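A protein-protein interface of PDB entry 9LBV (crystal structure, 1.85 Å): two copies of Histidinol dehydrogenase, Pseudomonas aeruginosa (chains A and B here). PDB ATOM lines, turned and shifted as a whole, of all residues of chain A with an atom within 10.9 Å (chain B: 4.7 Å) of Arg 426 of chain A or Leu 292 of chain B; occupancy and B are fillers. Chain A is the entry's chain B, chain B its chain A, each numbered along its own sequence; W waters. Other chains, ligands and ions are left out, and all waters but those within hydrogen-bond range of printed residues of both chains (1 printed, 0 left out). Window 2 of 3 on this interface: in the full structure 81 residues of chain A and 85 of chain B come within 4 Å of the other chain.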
ATOM      1  N   ALA A 405     -26.020  17.158  15.200  1.00  0.00           N
ATOM      2  CA  ALA A 405     -25.897  16.302  16.381  1.00  0.00           C
ATOM      3  C   ALA A 405     -24.693  15.379  16.272  1.00  0.00           C
ATOM      4  O   ALA A 405     -24.021  15.103  17.270  1.00  0.00           O
ATOM      5  CB  ALA A 405     -27.185  15.489  16.556  1.00  0.00           C
ATOM      6  N   LEU A 408     -21.421  17.724  16.755  1.00  0.00           N
ATOM      7  CA  LEU A 408     -21.297  18.136  18.146  1.00  0.00           C
ATOM      8  C   LEU A 408     -21.164  16.925  19.067  1.00  0.00           C
ATOM      9  O   LEU A 408     -20.471  16.993  20.084  1.00  0.00           O
ATOM     10  CB  LEU A 408     -22.497  18.993  18.536  1.00  0.00           C
ATOM     11  CG  LEU A 408     -22.680  20.295  17.734  1.00  0.00           C
ATOM     12  CD1 LEU A 408     -23.896  21.081  18.215  1.00  0.00           C
ATOM     13  CD2 LEU A 408     -21.451  21.155  17.851  1.00  0.00           C
ATOM     14  N   GLY A 409     -21.798  15.809  18.708  1.00  0.00           N
ATOM     15  CA  GLY A 409     -21.782  14.647  19.580  1.00  0.00           C
ATOM     16  C   GLY A 409     -20.403  14.045  19.710  1.00  0.00           C
ATOM     17  O   GLY A 409     -20.027  13.560  20.783  1.00  0.00           O
ATOM     18  N   ARG A 410     -19.620  14.074  18.622  1.00  0.00           N
ATOM     19  CA  ARG A 410     -18.266  13.525  18.700  1.00  0.00           C
ATOM     20  C   ARG A 410     -17.411  14.303  19.684  1.00  0.00           C
ATOM     21  O   ARG A 410     -16.632  13.717  20.442  1.00  0.00           O
ATOM     22  CB  ARG A 410     -17.609  13.533  17.322  1.00  0.00           C
ATOM     23  CG  ARG A 410     -18.339  12.673  16.315  1.00  0.00           C
ATOM     24  CD  ARG A 410     -17.694  12.775  14.931  1.00  0.00           C
ATOM     25  NE  ARG A 410     -18.710  12.772  13.885  1.00  0.00           N
ATOM     26  CZ  ARG A 410     -19.180  11.672  13.313  1.00  0.00           C
ATOM     27  NH1 ARG A 410     -18.762  10.469  13.682  1.00  0.00           N
ATOM     28  NH2 ARG A 410     -20.092  11.781  12.350  1.00  0.00           N
ATOM     29  N   THR A 411     -17.497  15.630  19.653  1.00  0.00           N
ATOM     30  CA  THR A 411     -16.718  16.437  20.587  1.00  0.00           C
ATOM     31  C   THR A 411     -17.220  16.255  22.018  1.00  0.00           C
ATOM     32  O   THR A 411     -16.428  16.112  22.949  1.00  0.00           O
ATOM     33  CB  THR A 411     -16.786  17.905  20.154  1.00  0.00           C
ATOM     34  OG1 THR A 411     -16.116  18.036  18.900  1.00  0.00           O
ATOM     35  CG2 THR A 411     -16.168  18.832  21.190  1.00  0.00           C
ATOM     36  N   ALA A 412     -18.534  16.229  22.205  1.00  0.00           N
ATOM     37  CA  ALA A 412     -19.083  15.941  23.518  1.00  0.00           C
ATOM     38  C   ALA A 412     -18.621  14.581  24.023  1.00  0.00           C
ATOM     39  O   ALA A 412     -18.267  14.437  25.200  1.00  0.00           O
ATOM     40  CB  ALA A 412     -20.602  16.008  23.449  1.00  0.00           C
ATOM     41  N   SER A 413     -18.596  13.573  23.139  1.00  0.00           N
ATOM     42  CA  SER A 413     -18.155  12.238  23.536  1.00  0.00           C
ATOM     43  C   SER A 413     -16.719  12.267  24.031  1.00  0.00           C
ATOM     44  O   SER A 413     -16.412  11.746  25.102  1.00  0.00           O
ATOM     45  CB  SER A 413     -18.280  11.253  22.367  1.00  0.00           C
ATOM     46  OG  SER A 413     -17.627  10.028  22.696  1.00  0.00           O
ATOM     47  N   VAL A 414     -15.821  12.867  23.251  1.00  0.00           N
ATOM     48  CA  VAL A 414     -14.407  12.915  23.619  1.00  0.00           C
ATOM     49  C   VAL A 414     -14.220  13.532  25.010  1.00  0.00           C
ATOM     50  O   VAL A 414     -13.499  13.000  25.861  1.00  0.00           O
ATOM     51  CB  VAL A 414     -13.625  13.704  22.553  1.00  0.00           C
ATOM     52  CG1 VAL A 414     -12.286  14.173  23.108  1.00  0.00           C
ATOM     53  CG2 VAL A 414     -13.446  12.841  21.286  1.00  0.00           C
ATOM     54  N   LEU A 415     -14.832  14.685  25.251  1.00  0.00           N
ATOM     55  CA  LEU A 415     -14.560  15.379  26.512  1.00  0.00           C
ATOM     56  C   LEU A 415     -15.283  14.714  27.691  1.00  0.00           C
ATOM     57  O   LEU A 415     -14.713  14.570  28.777  1.00  0.00           O
ATOM     58  CB  LEU A 415     -14.955  16.840  26.372  1.00  0.00           C
ATOM     59  CG  LEU A 415     -14.067  17.674  25.450  1.00  0.00           C
ATOM     60  CD1 LEU A 415     -14.617  19.096  25.327  1.00  0.00           C
ATOM     61  CD2 LEU A 415     -12.609  17.695  25.960  1.00  0.00           C
ATOM     62  N   ALA A 416     -16.536  14.299  27.501  1.00  0.00           N
ATOM     63  CA  ALA A 416     -17.258  13.612  28.579  1.00  0.00           C
ATOM     64  C   ALA A 416     -16.594  12.283  28.932  1.00  0.00           C
ATOM     65  O   ALA A 416     -16.410  11.971  30.112  1.00  0.00           O
ATOM     66  CB  ALA A 416     -18.720  13.380  28.188  1.00  0.00           C
ATOM     67  N   ARG A 417     -16.199  11.499  27.925  1.00  0.00           N
ATOM     68  CA  ARG A 417     -15.469  10.272  28.229  1.00  0.00           C
ATOM     69  C   ARG A 417     -14.157  10.584  28.930  1.00  0.00           C
ATOM     70  O   ARG A 417     -13.780   9.894  29.886  1.00  0.00           O
ATOM     71  CB  ARG A 417     -15.228   9.439  26.972  1.00  0.00           C
ATOM     72  CG  ARG A 417     -16.498   8.955  26.310  1.00  0.00           C
ATOM     73  CD  ARG A 417     -16.484   7.473  26.112  1.00  0.00           C
ATOM     74  NE  ARG A 417     -17.778   6.994  25.641  1.00  0.00           N
ATOM     75  CZ  ARG A 417     -18.357   5.891  26.096  1.00  0.00           C
ATOM     76  NH1 ARG A 417     -17.810   5.179  27.065  1.00  0.00           N
ATOM     77  NH2 ARG A 417     -19.521   5.502  25.575  1.00  0.00           N
ATOM     78  N   GLY A 418     -13.463  11.638  28.503  1.00  0.00           N
ATOM     79  CA  GLY A 418     -12.229  12.005  29.191  1.00  0.00           C
ATOM     80  C   GLY A 418     -12.426  12.257  30.677  1.00  0.00           C
ATOM     81  O   GLY A 418     -11.513  12.042  31.475  1.00  0.00           O
ATOM     82  N   SER A 420     -14.919  10.742  32.495  1.00  0.00           N
ATOM     83  CA  SER A 420     -15.656   9.606  33.050  1.00  0.00           C
ATOM     84  C   SER A 420     -17.127   9.931  33.305  1.00  0.00           C
ATOM     85  O   SER A 420     -17.799   9.231  34.058  1.00  0.00           O
ATOM     86  CB  SER A 420     -15.006   9.101  34.341  1.00  0.00           C
ATOM     87  OG  SER A 420     -13.719   8.584  34.081  1.00  0.00           O
ATOM     88  N   LEU A 421     -17.666  10.978  32.678  1.00  0.00           N
ATOM     89  CA  LEU A 421     -19.103  11.244  32.767  1.00  0.00           C
ATOM     90  C   LEU A 421     -19.801  10.538  31.603  1.00  0.00           C
ATOM     91  O   LEU A 421     -20.235  11.145  30.622  1.00  0.00           O
ATOM     92  CB  LEU A 421     -19.374  12.743  32.782  1.00  0.00           C
ATOM     93  CG  LEU A 421     -18.676  13.612  33.838  1.00  0.00           C
ATOM     94  CD1 LEU A 421     -19.300  15.016  33.892  1.00  0.00           C
ATOM     95  CD2 LEU A 421     -18.751  12.981  35.192  1.00  0.00           C
ATOM     96  N   THR A 422     -19.930   9.214  31.727  1.00  0.00           N
ATOM     97  CA  THR A 422     -20.312   8.400  30.575  1.00  0.00           C
ATOM     98  C   THR A 422     -21.792   8.487  30.225  1.00  0.00           C
ATOM     99  O   THR A 422     -22.171   8.071  29.122  1.00  0.00           O
ATOM    100  CB  THR A 422     -19.947   6.927  30.812  1.00  0.00           C
ATOM    101  OG1 THR A 422     -20.530   6.487  32.042  1.00  0.00           O
ATOM    102  CG2 THR A 422     -18.418   6.736  30.871  1.00  0.00           C
ATOM    103  N   ALA A 423     -22.655   8.955  31.139  1.00  0.00           N
ATOM    104  CA  ALA A 423     -24.037   9.189  30.716  1.00  0.00           C
ATOM    105  C   ALA A 423     -24.095  10.354  29.736  1.00  0.00           C
ATOM    106  O   ALA A 423     -24.805  10.292  28.725  1.00  0.00           O
ATOM    107  CB  ALA A 423     -24.940   9.458  31.923  1.00  0.00           C
ATOM    108  N   HIS A 424     -23.334  11.418  30.024  1.00  0.00           N
ATOM    109  CA  HIS A 424     -23.176  12.508  29.072  1.00  0.00           C
ATOM    110  C   HIS A 424     -22.696  11.968  27.724  1.00  0.00           C
ATOM    111  O   HIS A 424     -23.230  12.330  26.665  1.00  0.00           O
ATOM    112  CB  HIS A 424     -22.171  13.535  29.623  1.00  0.00           C
ATOM    113  CG  HIS A 424     -22.776  14.567  30.530  1.00  0.00           C
ATOM    114  ND1 HIS A 424     -23.025  14.330  31.867  1.00  0.00           N
ATOM    115  CD2 HIS A 424     -23.153  15.855  30.300  1.00  0.00           C
ATOM    116  CE1 HIS A 424     -23.545  15.416  32.416  1.00  0.00           C
ATOM    117  NE2 HIS A 424     -23.625  16.356  31.491  1.00  0.00           N
ATOM    118  N   ALA A 425     -21.670  11.107  27.746  1.00  0.00           N
ATOM    119  CA  ALA A 425     -21.088  10.613  26.499  1.00  0.00           C
ATOM    120  C   ALA A 425     -22.108   9.815  25.710  1.00  0.00           C
ATOM    121  O   ALA A 425     -22.362  10.103  24.531  1.00  0.00           O
ATOM    122  CB  ALA A 425     -19.854   9.755  26.790  1.00  0.00           C
ATOM    123  N   ARG A 426     -22.729   8.817  26.361  1.00  0.00           N
ATOM    124  CA  ARG A 426     -23.627   7.922  25.646  1.00  0.00           C
ATOM    125  C   ARG A 426     -24.855   8.667  25.143  1.00  0.00           C
ATOM    126  O   ARG A 426     -25.321   8.422  24.019  1.00  0.00           O
ATOM    127  CB  ARG A 426     -23.994   6.727  26.544  1.00  0.00           C
ATOM    128  CG  ARG A 426     -22.783   5.734  26.674  1.00  0.00           C
ATOM    129  CD  ARG A 426     -22.884   4.811  27.887  1.00  0.00           C
ATOM    130  NE  ARG A 426     -23.910   3.795  27.701  1.00  0.00           N
ATOM    131  CZ  ARG A 426     -24.206   2.856  28.589  1.00  0.00           C
ATOM    132  NH1 ARG A 426     -23.523   2.727  29.717  1.00  0.00           N
ATOM    133  NH2 ARG A 426     -25.232   2.045  28.355  1.00  0.00           N
ATOM    134  N   SER A 427     -25.366   9.616  25.944  1.00  0.00           N
ATOM    135  CA  SER A 427     -26.494  10.441  25.499  1.00  0.00           C
ATOM    136  C   SER A 427     -26.160  11.178  24.199  1.00  0.00           C
ATOM    137  O   SER A 427     -26.969  11.212  23.268  1.00  0.00           O
ATOM    138  CB  SER A 427     -26.858  11.434  26.615  1.00  0.00           C
ATOM    139  OG  SER A 427     -27.722  12.443  26.151  1.00  0.00           O
ATOM    140  N   ALA A 428     -24.949  11.740  24.110  1.00  0.00           N
ATOM    141  CA  ALA A 428     -24.511  12.395  22.878  1.00  0.00           C
ATOM    142  C   ALA A 428     -24.272  11.367  21.761  1.00  0.00           C
ATOM    143  O   ALA A 428     -24.665  11.583  20.611  1.00  0.00           O
ATOM    144  CB  ALA A 428     -23.235  13.186  23.155  1.00  0.00           C
ATOM    145  N   GLU A 429     -23.653  10.232  22.102  1.00  0.00           N
ATOM    146  CA  GLU A 429     -23.300   9.229  21.104  1.00  0.00           C
ATOM    147  C   GLU A 429     -24.517   8.598  20.463  1.00  0.00           C
ATOM    148  O   GLU A 429     -24.439   8.167  19.310  1.00  0.00           O
ATOM    149  CB  GLU A 429     -22.428   8.133  21.726  1.00  0.00           C
ATOM    150  CG  GLU A 429     -21.057   8.624  22.066  1.00  0.00           C
ATOM    151  CD  GLU A 429     -20.400   7.825  23.173  1.00  0.00           C
ATOM    152  OE1 GLU A 429     -21.006   6.849  23.669  1.00  0.00           O
ATOM    153  OE2 GLU A 429     -19.265   8.167  23.544  1.00  0.00           O
ATOM    154  N   TYR A 430     -25.642   8.534  21.180  1.00  0.00           N
ATOM    155  CA  TYR A 430     -26.838   7.920  20.604  1.00  0.00           C
ATOM    156  C   TYR A 430     -27.261   8.624  19.319  1.00  0.00           C
ATOM    157  O   TYR A 430     -27.919   8.021  18.466  1.00  0.00           O
ATOM    158  CB  TYR A 430     -28.006   7.975  21.593  1.00  0.00           C
ATOM    159  CG  TYR A 430     -28.132   6.820  22.561  1.00  0.00           C
ATOM    160  CD1 TYR A 430     -28.156   5.487  22.124  1.00  0.00           C
ATOM    161  CD2 TYR A 430     -28.284   7.070  23.926  1.00  0.00           C
ATOM    162  CE1 TYR A 430     -28.289   4.448  23.034  1.00  0.00           C
ATOM    163  CE2 TYR A 430     -28.418   6.034  24.837  1.00  0.00           C
ATOM    164  CZ  TYR A 430     -28.429   4.731  24.385  1.00  0.00           C
ATOM    165  OH  TYR A 430     -28.569   3.713  25.306  1.00  0.00           O
ATOM    166  N   ARG A 431     -26.938   9.906  19.176  1.00  0.00           N
ATOM    167  CA  ARG A 431     -27.396  10.684  18.034  1.00  0.00           C
ATOM    168  C   ARG A 431     -26.362  10.762  16.922  1.00  0.00           C
ATOM    169  O   ARG A 431     -26.621  11.418  15.909  1.00  0.00           O
ATOM    170  CB  ARG A 431     -27.769  12.112  18.472  1.00  0.00           C
ATOM    171  CG  ARG A 431     -29.173  12.238  19.071  1.00  0.00           C
ATOM    172  CD  ARG A 431     -29.168  11.936  20.572  1.00  0.00           C
ATOM    173  NE  ARG A 431     -30.425  12.356  21.205  1.00  0.00           N
ATOM    174  CZ  ARG A 431     -30.696  12.251  22.500  1.00  0.00           C
ATOM    175  NH1 ARG A 431     -29.810  11.761  23.361  1.00  0.00           N
ATOM    176  NH2 ARG A 431     -31.883  12.638  22.945  1.00  0.00           N
ATOM    177  N   ILE A 432     -25.177  10.178  17.103  1.00  0.00           N
ATOM    178  CA  ILE A 432     -24.184  10.244  16.039  1.00  0.00           C
ATOM    179  C   ILE A 432     -24.619   9.320  14.910  1.00  0.00           C
ATOM    180  O   ILE A 432     -24.964   8.156  15.140  1.00  0.00           O
ATOM    181  CB  ILE A 432     -22.794   9.874  16.556  1.00  0.00           C
ATOM    182  CG1 ILE A 432     -22.345  10.835  17.652  1.00  0.00           C
ATOM    183  CG2 ILE A 432     -21.782   9.888  15.400  1.00  0.00           C
ATOM    184  CD1 ILE A 432     -21.002  10.441  18.253  1.00  0.00           C
ATOM    185  N   LEU A 433     -24.619   9.832  13.686  1.00  0.00           N
ATOM    186  CA  LEU A 433     -25.112   9.060  12.560  1.00  0.00           C
ATOM    187  C   LEU A 433     -23.965   8.736  11.611  1.00  0.00           C
ATOM    188  O   LEU A 433     -23.134   9.597  11.306  1.00  0.00           O
ATOM    189  CB  LEU A 433     -26.241   9.799  11.846  1.00  0.00           C
ATOM    190  CG  LEU A 433     -27.636   9.230  12.148  1.00  0.00           C
ATOM    191  CD1 LEU A 433     -28.728  10.172  11.624  1.00  0.00           C
ATOM    192  CD2 LEU A 433     -27.860   7.784  11.647  1.00  0.00           C
ATOM    193  N   ASP B 254     -34.372   4.529  25.322  1.00  0.00           N
ATOM    194  CA  ASP B 254     -33.012   4.486  25.844  1.00  0.00           C
ATOM    195  C   ASP B 254     -32.373   5.865  25.789  1.00  0.00           C
ATOM    196  O   ASP B 254     -31.671   6.264  26.728  1.00  0.00           O
ATOM    197  CB  ASP B 254     -32.157   3.502  25.048  1.00  0.00           C
ATOM    198  CG  ASP B 254     -32.652   2.063  25.167  1.00  0.00           C
ATOM    199  OD1 ASP B 254     -33.295   1.736  26.193  1.00  0.00           O
ATOM    200  OD2 ASP B 254     -32.395   1.281  24.222  1.00  0.00           O
ATOM    201  N   ALA B 257     -33.942   7.819  28.626  1.00  0.00           N
ATOM    202  CA  ALA B 257     -33.326   7.362  29.872  1.00  0.00           C
ATOM    203  C   ALA B 257     -31.935   7.952  30.039  1.00  0.00           C
ATOM    204  O   ALA B 257     -31.586   8.458  31.112  1.00  0.00           O
ATOM    205  CB  ALA B 257     -33.247   5.833  29.907  1.00  0.00           C
ATOM    206  N   MET B 258     -31.120   7.888  28.983  1.00  0.00           N
ATOM    207  CA  MET B 258     -29.735   8.364  29.101  1.00  0.00           C
ATOM    208  C   MET B 258     -29.688   9.878  29.296  1.00  0.00           C
ATOM    209  O   MET B 258     -28.798  10.406  29.998  1.00  0.00           O
ATOM    210  CB  MET B 258     -28.927   7.983  27.859  1.00  0.00           C
ATOM    211  CG  MET B 258     -27.412   7.926  28.115  1.00  0.00           C
ATOM    212  SD  MET B 258     -26.861   6.865  29.437  1.00  0.00           S
ATOM    213  CE  MET B 258     -27.394   5.245  28.797  1.00  0.00           C
ATOM    214  N   PHE B 261     -30.203  10.366  32.825  1.00  0.00           N
ATOM    215  CA  PHE B 261     -28.977   9.966  33.528  1.00  0.00           C
ATOM    216  C   PHE B 261     -27.884  11.017  33.404  1.00  0.00           C
ATOM    217  O   PHE B 261     -27.056  11.169  34.304  1.00  0.00           O
ATOM    218  CB  PHE B 261     -28.405   8.669  32.940  1.00  0.00           C
ATOM    219  CG  PHE B 261     -29.126   7.395  33.340  1.00  0.00           C
ATOM    220  CD1 PHE B 261     -30.325   7.409  34.029  1.00  0.00           C
ATOM    221  CD2 PHE B 261     -28.578   6.169  32.990  1.00  0.00           C
ATOM    222  CE1 PHE B 261     -30.969   6.183  34.375  1.00  0.00           C
ATOM    223  CE2 PHE B 261     -29.205   4.961  33.329  1.00  0.00           C
ATOM    224  CZ  PHE B 261     -30.404   4.985  34.023  1.00  0.00           C
ATOM    225  N   SER B 288     -36.150   1.058  30.380  1.00  0.00           N
ATOM    226  CA  SER B 288     -34.798   1.477  29.984  1.00  0.00           C
ATOM    227  C   SER B 288     -33.976   1.910  31.187  1.00  0.00           C
ATOM    228  O   SER B 288     -32.804   1.530  31.320  1.00  0.00           O
ATOM    229  CB  SER B 288     -34.852   2.601  28.949  1.00  0.00           C
ATOM    230  OG  SER B 288     -35.419   2.159  27.725  1.00  0.00           O
ATOM    231  N   ILE B 289     -34.578   2.684  32.092  1.00  0.00           N
ATOM    232  CA  ILE B 289     -33.861   3.096  33.297  1.00  0.00           C
ATOM    233  C   ILE B 289     -33.390   1.869  34.073  1.00  0.00           C
ATOM    234  O   ILE B 289     -32.215   1.754  34.455  1.00  0.00           O
ATOM    235  CB  ILE B 289     -34.756   4.012  34.159  1.00  0.00           C
ATOM    236  CG1 ILE B 289     -34.910   5.400  33.509  1.00  0.00           C
ATOM    237  CG2 ILE B 289     -34.204   4.135  35.576  1.00  0.00           C
ATOM    238  CD1 ILE B 289     -35.871   6.324  34.275  1.00  0.00           C
ATOM    239  N   ALA B 290     -34.308   0.922  34.306  1.00  0.00           N
ATOM    240  CA  ALA B 290     -33.981  -0.247  35.112  1.00  0.00           C
ATOM    241  C   ALA B 290     -32.838  -1.033  34.496  1.00  0.00           C
ATOM    242  O   ALA B 290     -31.936  -1.487  35.206  1.00  0.00           O
ATOM    243  CB  ALA B 290     -35.222  -1.132  35.264  1.00  0.00           C
ATOM    244  N   ARG B 291     -32.863  -1.192  33.169  1.00  0.00           N
ATOM    245  CA  ARG B 291     -31.855  -1.980  32.469  1.00  0.00           C
ATOM    246  C   ARG B 291     -30.522  -1.251  32.373  1.00  0.00           C
ATOM    247  O   ARG B 291     -29.475  -1.853  32.607  1.00  0.00           O
ATOM    248  CB  ARG B 291     -32.355  -2.360  31.065  1.00  0.00           C
ATOM    249  CG  ARG B 291     -31.327  -3.208  30.298  1.00  0.00           C
ATOM    250  CD  ARG B 291     -31.801  -3.658  28.914  1.00  0.00           C
ATOM    251  NE  ARG B 291     -31.525  -2.673  27.873  1.00  0.00           N
ATOM    252  CZ  ARG B 291     -32.449  -1.903  27.312  1.00  0.00           C
ATOM    253  NH1 ARG B 291     -33.716  -1.961  27.694  1.00  0.00           N
ATOM    254  NH2 ARG B 291     -32.094  -1.067  26.334  1.00  0.00           N
ATOM    255  N   LEU B 292     -30.537   0.047  32.046  1.00  0.00           N
ATOM    256  CA  LEU B 292     -29.303   0.784  31.754  1.00  0.00           C
ATOM    257  C   LEU B 292     -28.563   1.207  33.009  1.00  0.00           C
ATOM    258  O   LEU B 292     -27.341   1.396  32.966  1.00  0.00           O
ATOM    259  CB  LEU B 292     -29.631   2.027  30.912  1.00  0.00           C
ATOM    260  CG  LEU B 292     -30.106   1.677  29.507  1.00  0.00           C
ATOM    261  CD1 LEU B 292     -30.580   2.915  28.743  1.00  0.00           C
ATOM    262  CD2 LEU B 292     -28.984   0.958  28.752  1.00  0.00           C
ATOM    263  N   LEU B 293     -29.269   1.368  34.123  1.00  0.00           N
ATOM    264  CA  LEU B 293     -28.641   1.925  35.324  1.00  0.00           C
ATOM    265  C   LEU B 293     -27.448   1.114  35.817  1.00  0.00           C
ATOM    266  O   LEU B 293     -26.404   1.721  36.126  1.00  0.00           O
ATOM    267  CB  LEU B 293     -29.692   2.081  36.428  1.00  0.00           C
ATOM    268  CG  LEU B 293     -29.120   2.545  37.767  1.00  0.00           C
ATOM    269  CD1 LEU B 293     -28.478   3.927  37.607  1.00  0.00           C
ATOM    270  CD2 LEU B 293     -30.183   2.568  38.889  1.00  0.00           C
ATOM    271  N   PRO B 294     -27.511  -0.224  35.937  1.00  0.00           N
ATOM    272  CA  PRO B 294     -26.326  -0.940  36.432  1.00  0.00           C
ATOM    273  C   PRO B 294     -25.165  -0.918  35.460  1.00  0.00           C
ATOM    274  O   PRO B 294     -24.032  -1.167  35.882  1.00  0.00           O
ATOM    275  CB  PRO B 294     -26.838  -2.368  36.679  1.00  0.00           C
ATOM    276  CG  PRO B 294     -28.040  -2.504  35.810  1.00  0.00           C
ATOM    277  CD  PRO B 294     -28.678  -1.123  35.820  1.00  0.00           C
ATOM    278  N   THR B 295     -25.398  -0.610  34.185  1.00  0.00           N
ATOM    279  CA  THR B 295     -24.316  -0.462  33.221  1.00  0.00           C
ATOM    280  C   THR B 295     -23.589   0.884  33.316  1.00  0.00           C
ATOM    281  O   THR B 295     -22.648   1.104  32.542  1.00  0.00           O
ATOM    282  CB  THR B 295     -24.861  -0.628  31.803  1.00  0.00           C
ATOM    283  OG1 THR B 295     -25.479   0.596  31.379  1.00  0.00           O
ATOM    284  CG2 THR B 295     -25.902  -1.737  31.760  1.00  0.00           C
ATOM    285  N   MET B 296     -23.997   1.794  34.205  1.00  0.00           N
ATOM    286  CA  MET B 296     -23.420   3.141  34.261  1.00  0.00           C
ATOM    287  C   MET B 296     -22.270   3.209  35.259  1.00  0.00           C
ATOM    288  O   MET B 296     -22.421   2.800  36.412  1.00  0.00           O
ATOM    289  CB  MET B 296     -24.482   4.173  34.645  1.00  0.00           C
ATOM    290  CG  MET B 296     -25.725   4.175  33.748  1.00  0.00           C
ATOM    291  SD  MET B 296     -25.355   4.175  31.968  1.00  0.00           S
ATOM    292  CE  MET B 296     -24.265   5.611  31.811  1.00  0.00           C
HETATM  293  O   HOH W   1     -29.537   1.472  24.065  1.00  0.00           O
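No position is printed for both chains.
Of the 11 pairs that touch across the chains among the printed residues, none has its exchanged pair printed and touching as well.
OD1 of Asp 254 of chain B lies within salt-bridge range of NH2 of Arg 291 of chain B (3.1 Å).
The side-chain sulfur of Met 296 of chain B sits at hydrogen-bond distance from the side-chain hydroxyl of Thr 295 of chain B (3.6 Å).
OD1 of Asp 254 of chain B lies within hydrogen-bond range of OG of Ser 288 of chain B.
O of Leu 292 of chain B lies within hydrogen-bond range of OG1 of Thr 295 of chain B (2.6 Å).
The guanidinium group (NH1) of Arg 431 of chain A lies within hydrogen-bond range of the backbone carbonyl oxygen (O) of Ser 427 of chain A (2.9 Å).
Of the 26 printed residues of chain A, 5 touch a printed residue of chain B.
Of the 13 printed residues of chain B, 6 touch a printed residue of chain A.
Hydrophobic or aromatic side chains of chain B within 4 Å of the printed part of chain A: Met 258, Phe 261, Leu 292 and Met 296.
Among the printed residues, 11 pairs touch across the chains.
Among the printed residues, no Asp or Glu carboxylate lies within 4 Å of a Lys or Arg side-chain nitrogen of the other chain.
Water W1 lies within hydrogen-bond range of the side-chain hydroxyl (OH) of Tyr 430 of chain A (2.7 Å) and the side-chain carboxylate (OD2) of Asp 254 of chain B (2.9 Å).
Printed residues of chain B within 4 Å of Thr 422 of chain A: Met 296 (3.8 Å).
Of chain B, only Met 258, Leu 292, Thr 295 and Met 296 come within 4 Å of Arg 426 of chain A.
Of the printed residues of chain B, Ser 427 of chain A touches Met 258 (3.4 Å).
Of chain A, only Tyr 430 (3.6 Å) comes within 4 Å of Asp 254 of chain B.
No residue of chain A comes within 4 Å of Ala 257 of chain B.
Of the printed residues of chain A, Met 258 of chain B touches Ala 423, Arg 426, Ser 427 and Tyr 430.
Of the printed residues of chain A, Phe 261 of chain B touches Ala 423 (3.6 Å).
No residue of chain A comes within 4 Å of Ser 288 of chain B.
No residue of chain A comes within 4 Å of Ala 290 of chain B.
Arg 291 of chain B touches none of the printed residues of chain A.
Of chain A, only Arg 426 comes within 4 Å of Leu 292 of chain B.
Leu 293 of chain B touches none of the printed residues of chain A.
Pro 294 of chain B touches none of the printed residues of chain A.
Thr 295 of chain B touches just one residue of chain A: Arg 426 (3.3 Å).
Met 296 of chain B touches just these residues of chain A: Thr 422 (3.8 Å), Ala 423 (3.7 Å) and Arg 426 (3.2 Å).
The nearest printed residue of chain B that does not touch Arg 426 of chain A is Phe 261 of chain B (6.9 Å).
The nearest residue of chain A that does not touch Leu 292 of chain B is Tyr 430 of chain A (4.1 Å).
The nearest printed residue of chain B that does not touch Ala 423 of chain A is Ala 257 of chain B (6.8 Å).
The guanidinium group (NH1) of Arg 426 of chain A lies within hydrogen-bond range of the side-chain sulfur (SD) of Met 296 of chain B, at 3.2 Å.
The guanidinium group of Arg 426 of chain A is in hydrogen-bond range of the side-chain hydroxyl of Thr 295 of chain B (3.3 Å).
Met 296 of chain B touches Thr 422 of chain A (CE to OG1, 3.8 Å).
CG of Met 258 of chain B touches O of Ala 423 of chain A, 3.6 Å away.
Phe 261 of chain B touches Ala 423 of chain A.
CE of Met 296 of chain B touches CA of Ala 423 of chain A (3.7 Å).
Met 258 of chain B touches Arg 426 of chain A (CE to NH2, 3.9 Å).
NH2 of Arg 426 of chain A touches CD2 of Leu 292 of chain B (3.9 Å).
N of Ser 427 of chain A touches CG of Met 258 of chain B, at 3.4 Å.
CB of Asp 254 of chain B touches OH of Tyr 430 of chain A, 3.6 Å away.
Met 258 of chain B touches Tyr 430 of chain A.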
